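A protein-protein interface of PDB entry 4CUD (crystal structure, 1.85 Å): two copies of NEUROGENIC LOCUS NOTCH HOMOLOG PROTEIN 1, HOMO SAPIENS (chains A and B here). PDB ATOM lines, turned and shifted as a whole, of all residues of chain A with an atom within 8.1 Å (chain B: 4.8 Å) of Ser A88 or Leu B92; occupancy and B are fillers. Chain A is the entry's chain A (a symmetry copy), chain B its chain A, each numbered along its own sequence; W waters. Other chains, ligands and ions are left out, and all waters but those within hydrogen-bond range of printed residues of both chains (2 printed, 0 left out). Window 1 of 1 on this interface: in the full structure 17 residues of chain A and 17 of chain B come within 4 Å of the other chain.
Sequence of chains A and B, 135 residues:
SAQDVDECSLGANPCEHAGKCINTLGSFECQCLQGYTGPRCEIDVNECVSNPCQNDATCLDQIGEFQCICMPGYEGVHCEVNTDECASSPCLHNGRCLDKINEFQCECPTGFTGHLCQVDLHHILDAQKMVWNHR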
ATOM      1  N   ASP A  84      13.180  12.080 -24.942  1.00  0.00           N
ATOM      2  CA  ASP A  84      12.375  13.285 -24.804  1.00  0.00           C
ATOM      3  C   ASP A  84      13.056  14.223 -23.810  1.00  0.00           C
ATOM      4  O   ASP A  84      12.920  14.066 -22.604  1.00  0.00           O
ATOM      5  CB  ASP A  84      10.946  12.924 -24.369  1.00  0.00           C
ATOM      6  CG  ASP A  84      10.020  14.135 -24.275  1.00  0.00           C
ATOM      7  OD1 ASP A  84      10.385  15.246 -24.717  1.00  0.00           O
ATOM      8  OD2 ASP A  84       8.900  13.963 -23.747  1.00  0.00           O
ATOM      9  N   GLU A  85      13.817  15.189 -24.326  1.00  0.00           N
ATOM     10  CA  GLU A  85      14.474  16.171 -23.463  1.00  0.00           C
ATOM     11  C   GLU A  85      13.477  17.075 -22.728  1.00  0.00           C
ATOM     12  O   GLU A  85      13.852  17.799 -21.809  1.00  0.00           O
ATOM     13  CB  GLU A  85      15.509  16.993 -24.236  1.00  0.00           C
ATOM     14  CG  GLU A  85      16.818  16.247 -24.497  1.00  0.00           C
ATOM     15  CD  GLU A  85      16.767  15.321 -25.700  1.00  0.00           C
ATOM     16  OE1 GLU A  85      15.961  15.559 -26.621  1.00  0.00           O
ATOM     17  OE2 GLU A  85      17.552  14.351 -25.748  1.00  0.00           O
ATOM     18  N   CYS A  86      12.211  17.019 -23.128  1.00  0.00           N
ATOM     19  CA  CYS A  86      11.186  17.820 -22.467  1.00  0.00           C
ATOM     20  C   CYS A  86      10.613  17.138 -21.231  1.00  0.00           C
ATOM     21  O   CYS A  86       9.915  17.778 -20.435  1.00  0.00           O
ATOM     22  CB  CYS A  86      10.083  18.213 -23.454  1.00  0.00           C
ATOM     23  SG  CYS A  86      10.713  19.351 -24.711  1.00  0.00           S
ATOM     24  N   ALA A  87      10.923  15.853 -21.067  1.00  0.00           N
ATOM     25  CA  ALA A  87      10.365  15.045 -19.986  1.00  0.00           C
ATOM     26  C   ALA A  87      10.626  15.620 -18.582  1.00  0.00           C
ATOM     27  O   ALA A  87       9.783  15.480 -17.697  1.00  0.00           O
ATOM     28  CB  ALA A  87      10.860  13.608 -20.082  1.00  0.00           C
ATOM     29  N   SER A  88      11.767  16.287 -18.389  1.00  0.00           N
ATOM     30  CA  SER A  88      12.099  16.883 -17.083  1.00  0.00           C
ATOM     31  C   SER A  88      11.549  18.307 -16.883  1.00  0.00           C
ATOM     32  O   SER A  88      11.864  18.960 -15.887  1.00  0.00           O
ATOM     33  CB  SER A  88      13.618  16.856 -16.845  1.00  0.00           C
ATOM     34  OG  SER A  88      14.285  17.790 -17.687  1.00  0.00           O
ATOM     35  N   SER A  89      10.720  18.770 -17.817  1.00  0.00           N
ATOM     36  CA  SER A  89      10.145  20.133 -17.798  1.00  0.00           C
ATOM     37  C   SER A  89      11.216  21.215 -17.589  1.00  0.00           C
ATOM     38  O   SER A  89      11.176  21.952 -16.598  1.00  0.00           O
ATOM     39  CB  SER A  89       9.039  20.277 -16.733  1.00  0.00           C
ATOM     40  OG  SER A  89       8.184  19.149 -16.677  1.00  0.00           O
ATOM     41  N   PRO A  90      12.182  21.315 -18.516  1.00  0.00           N
ATOM     42  CA  PRO A  90      13.279  22.272 -18.318  1.00  0.00           C
ATOM     43  C   PRO A  90      12.878  23.736 -18.534  1.00  0.00           C
ATOM     44  O   PRO A  90      13.606  24.638 -18.104  1.00  0.00           O
ATOM     45  CB  PRO A  90      14.306  21.840 -19.361  1.00  0.00           C
ATOM     46  CG  PRO A  90      13.503  21.208 -20.444  1.00  0.00           C
ATOM     47  CD  PRO A  90      12.299  20.588 -19.795  1.00  0.00           C
ATOM     48  N   CYS A  91      11.754  23.975 -19.208  1.00  0.00           N
ATOM     49  CA  CYS A  91      11.318  25.347 -19.489  1.00  0.00           C
ATOM     50  C   CYS A  91      10.571  25.913 -18.295  1.00  0.00           C
ATOM     51  O   CYS A  91       9.561  25.341 -17.858  1.00  0.00           O
ATOM     52  CB  CYS A  91      10.426  25.418 -20.726  1.00  0.00           C
ATOM     53  SG  CYS A  91      11.114  24.677 -22.219  1.00  0.00           S
ATOM     54  N   CYS A  97       7.756  23.424 -24.315  1.00  0.00           N
ATOM     55  CA  CYS A  97       9.000  22.723 -24.638  1.00  0.00           C
ATOM     56  C   CYS A  97       8.872  21.964 -25.958  1.00  0.00           C
ATOM     57  O   CYS A  97       7.929  21.186 -26.161  1.00  0.00           O
ATOM     58  CB  CYS A  97       9.422  21.793 -23.493  1.00  0.00           C
ATOM     59  SG  CYS A  97      11.075  21.062 -23.674  1.00  0.00           S
ATOM     60  N   PHE A 104      16.581  20.686 -26.847  1.00  0.00           N
ATOM     61  CA  PHE A 104      15.193  21.130 -26.750  1.00  0.00           C
ATOM     62  C   PHE A 104      15.148  22.643 -26.937  1.00  0.00           C
ATOM     63  O   PHE A 104      16.167  23.326 -26.787  1.00  0.00           O
ATOM     64  CB  PHE A 104      14.582  20.742 -25.389  1.00  0.00           C
ATOM     65  CG  PHE A 104      15.239  21.427 -24.217  1.00  0.00           C
ATOM     66  CD1 PHE A 104      14.768  22.658 -23.761  1.00  0.00           C
ATOM     67  CD2 PHE A 104      16.329  20.844 -23.573  1.00  0.00           C
ATOM     68  CE1 PHE A 104      15.380  23.307 -22.696  1.00  0.00           C
ATOM     69  CE2 PHE A 104      16.947  21.485 -22.510  1.00  0.00           C
ATOM     70  CZ  PHE A 104      16.475  22.717 -22.071  1.00  0.00           C
ATOM     71  N   PRO B  90      19.209  22.234 -14.411  1.00  0.00           N
ATOM     72  CA  PRO B  90      18.601  21.430 -15.480  1.00  0.00           C
ATOM     73  C   PRO B  90      19.210  20.031 -15.635  1.00  0.00           C
ATOM     74  O   PRO B  90      18.596  19.165 -16.268  1.00  0.00           O
ATOM     75  CB  PRO B  90      18.861  22.266 -16.730  1.00  0.00           C
ATOM     76  CG  PRO B  90      20.097  23.035 -16.422  1.00  0.00           C
ATOM     77  CD  PRO B  90      20.107  23.280 -14.940  1.00  0.00           C
ATOM     78  N   CYS B  91      20.406  19.815 -15.088  1.00  0.00           N
ATOM     79  CA  CYS B  91      21.073  18.516 -15.220  1.00  0.00           C
ATOM     80  C   CYS B  91      20.559  17.553 -14.165  1.00  0.00           C
ATOM     81  O   CYS B  91      20.647  17.836 -12.961  1.00  0.00           O
ATOM     82  CB  CYS B  91      22.590  18.641 -15.097  1.00  0.00           C
ATOM     83  SG  CYS B  91      23.359  19.840 -16.202  1.00  0.00           S
ATOM     84  N   LEU B  92      20.025  16.427 -14.624  1.00  0.00           N
ATOM     85  CA  LEU B  92      19.480  15.411 -13.727  1.00  0.00           C
ATOM     86  C   LEU B  92      20.620  14.598 -13.126  1.00  0.00           C
ATOM     87  O   LEU B  92      21.750  14.637 -13.621  1.00  0.00           O
ATOM     88  CB  LEU B  92      18.484  14.491 -14.463  1.00  0.00           C
ATOM     89  CG  LEU B  92      17.215  15.069 -15.121  1.00  0.00           C
ATOM     90  CD1 LEU B  92      16.428  13.949 -15.784  1.00  0.00           C
ATOM     91  CD2 LEU B  92      16.333  15.831 -14.138  1.00  0.00           C
ATOM     92  N   HIS B  93      20.316  13.878 -12.045  1.00  0.00           N
ATOM     93  CA  HIS B  93      21.254  12.944 -11.403  1.00  0.00           C
ATOM     94  C   HIS B  93      22.578  13.532 -10.998  1.00  0.00           C
ATOM     95  O   HIS B  93      23.624  12.886 -11.142  1.00  0.00           O
ATOM     96  CB  HIS B  93      21.446  11.700 -12.267  1.00  0.00           C
ATOM     97  CG  HIS B  93      20.163  10.958 -12.542  1.00  0.00           C
ATOM     98  ND1 HIS B  93      19.565  10.963 -13.749  1.00  0.00           N
ATOM     99  CD2 HIS B  93      19.352  10.196 -11.705  1.00  0.00           C
ATOM    100  CE1 HIS B  93      18.435  10.238 -13.692  1.00  0.00           C
ATOM    101  NE2 HIS B  93      18.300   9.773 -12.439  1.00  0.00           N
ATOM    102  N   ASN B  94      22.543  14.755 -10.474  1.00  0.00           N
ATOM    103  CA  ASN B  94      23.742  15.435  -9.981  1.00  0.00           C
ATOM    104  C   ASN B  94      24.788  15.679 -11.060  1.00  0.00           C
ATOM    105  O   ASN B  94      25.974  15.751 -10.762  1.00  0.00           O
ATOM    106  CB  ASN B  94      24.370  14.668  -8.808  1.00  0.00           C
ATOM    107  CG  ASN B  94      23.381  14.387  -7.701  1.00  0.00           C
ATOM    108  OD1 ASN B  94      22.783  13.310  -7.652  1.00  0.00           O
ATOM    109  ND2 ASN B  94      23.178  15.364  -6.823  1.00  0.00           N
ATOM    110  N   GLY B  95      24.349  15.806 -12.311  1.00  0.00           N
ATOM    111  CA  GLY B  95      25.255  16.184 -13.397  1.00  0.00           C
ATOM    112  C   GLY B  95      25.832  17.560 -13.131  1.00  0.00           C
ATOM    113  O   GLY B  95      25.146  18.430 -12.594  1.00  0.00           O
ATOM    114  N   LEU B 116      20.694  16.091 -20.739  1.00  0.00           N
ATOM    115  CA  LEU B 116      20.237  16.434 -19.396  1.00  0.00           C
ATOM    116  C   LEU B 116      20.487  15.285 -18.422  1.00  0.00           C
ATOM    117  O   LEU B 116      19.900  15.243 -17.339  1.00  0.00           O
ATOM    118  CB  LEU B 116      18.742  16.797 -19.429  1.00  0.00           C
ATOM    119  CG  LEU B 116      18.373  17.999 -20.307  1.00  0.00           C
ATOM    120  CD1 LEU B 116      16.912  18.402 -20.166  1.00  0.00           C
ATOM    121  CD2 LEU B 116      19.261  19.172 -19.959  1.00  0.00           C
ATOM    122  N   CYS B 117      21.358  14.356 -18.825  1.00  0.00           N
ATOM    123  CA  CYS B 117      21.708  13.182 -18.023  1.00  0.00           C
ATOM    124  C   CYS B 117      20.501  12.285 -17.729  1.00  0.00           C
ATOM    125  O   CYS B 117      20.478  11.580 -16.722  1.00  0.00           O
ATOM    126  CB  CYS B 117      22.407  13.614 -16.726  1.00  0.00           C
ATOM    127  SG  CYS B 117      23.894  14.600 -17.023  1.00  0.00           S
ATOM    128  N   GLN B 118      19.519  12.316 -18.632  1.00  0.00           N
ATOM    129  CA  GLN B 118      18.253  11.583 -18.500  1.00  0.00           C
ATOM    130  C   GLN B 118      18.375  10.087 -18.634  1.00  0.00           C
ATOM    131  O   GLN B 118      17.608   9.339 -18.020  1.00  0.00           O
ATOM    132  CB  GLN B 118      17.313  11.974 -19.629  1.00  0.00           C
ATOM    133  CG  GLN B 118      16.441  13.172 -19.391  1.00  0.00           C
ATOM    134  CD  GLN B 118      15.656  13.487 -20.636  1.00  0.00           C
ATOM    135  OE1 GLN B 118      15.982  14.423 -21.346  1.00  0.00           O
ATOM    136  NE2 GLN B 118      14.649  12.669 -20.935  1.00  0.00           N
HETATM  137  O   HOH W   1      15.905  19.206 -16.155  1.00  0.00           O
HETATM  138  O   HOH W   2      14.474  16.123 -19.589  1.00  0.00           O
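Printed residues of chain B within 4 Å of Asp A84: Gln B118.
Of the printed residues of chain B, Glu A85 touches Leu B116 and Gln B118.
Printed residues of chain B within 4 Å of Ala A87: Gln B118.
Ser A88 touches just these residues of chain B: Leu B92 (3.97 Å) and Leu B116 (3.7 Å).
Cys A91 touches none of the printed residues of chain B.
Of chain A, only Ser A88 comes within 4 Å of Leu B92.
His B93 touches none of the printed residues of chain A.
Of the printed residues of chain A, Leu B116 touches Glu A85 (3.5 Å), Ser A88 (3.7 Å) and Phe A104 (3.9 Å).
Printed residues of chain A within 4 Å of Gln B118: Asp A84 (2.8 Å), Glu A85 (3.1 Å) and Ala A87 (3.996 Å).
The nearest residue of chain A that does not touch Leu B92 is Ala A87 (6.7 Å).
The backbone carbonyl oxygen of Asp A84 lies within hydrogen-bond range of the side-chain amide nitrogen of Gln B118.
Water W2 lies within hydrogen-bond range of OG of Ser A88 (2.5 Å), O of Glu A85 (2.9 Å) and OE1 of Gln B118 (2.9 Å).
Water W1 bridges OG of Ser A88 (2.6 Å) and O of Pro B90 (2.7 Å).
Of the 9 printed residues of chain B, 3 touch a printed residue of chain A.
Hydrophobic or aromatic side chains of chain B that line the printed part of chain A: Leu B92 and Leu B116.
Hydrophobic or aromatic side chains of chain A within 4 Å of the printed part of chain B: Ala A87 and Phe A104.
Among the printed residues, 7 pairs touch across the chains.
OD1 of Asp A84 sits close to N of Cys A86 (3.0 Å).
N of Leu B92 is in hydrogen-bond range of O of Leu B116 (3.0 Å).
The side-chain sulfur of Cys A86 forms a disulfide with the side-chain sulfur of Cys A97, 2.0 Å away.
Positions printed for both chains: 90 and 91.
Among the printed residues, merely in contact across the chains: Glu A85 with Leu B116 (3.5 Å), Glu A85 with Gln B118 (3.1 Å), Ala A87 with Gln B118 (3.996 Å), Ser A88 with Leu B92 (3.97 Å), Ser A88 with Leu B116 (3.7 Å) and Phe A104 with Leu B116 (3.9 Å).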
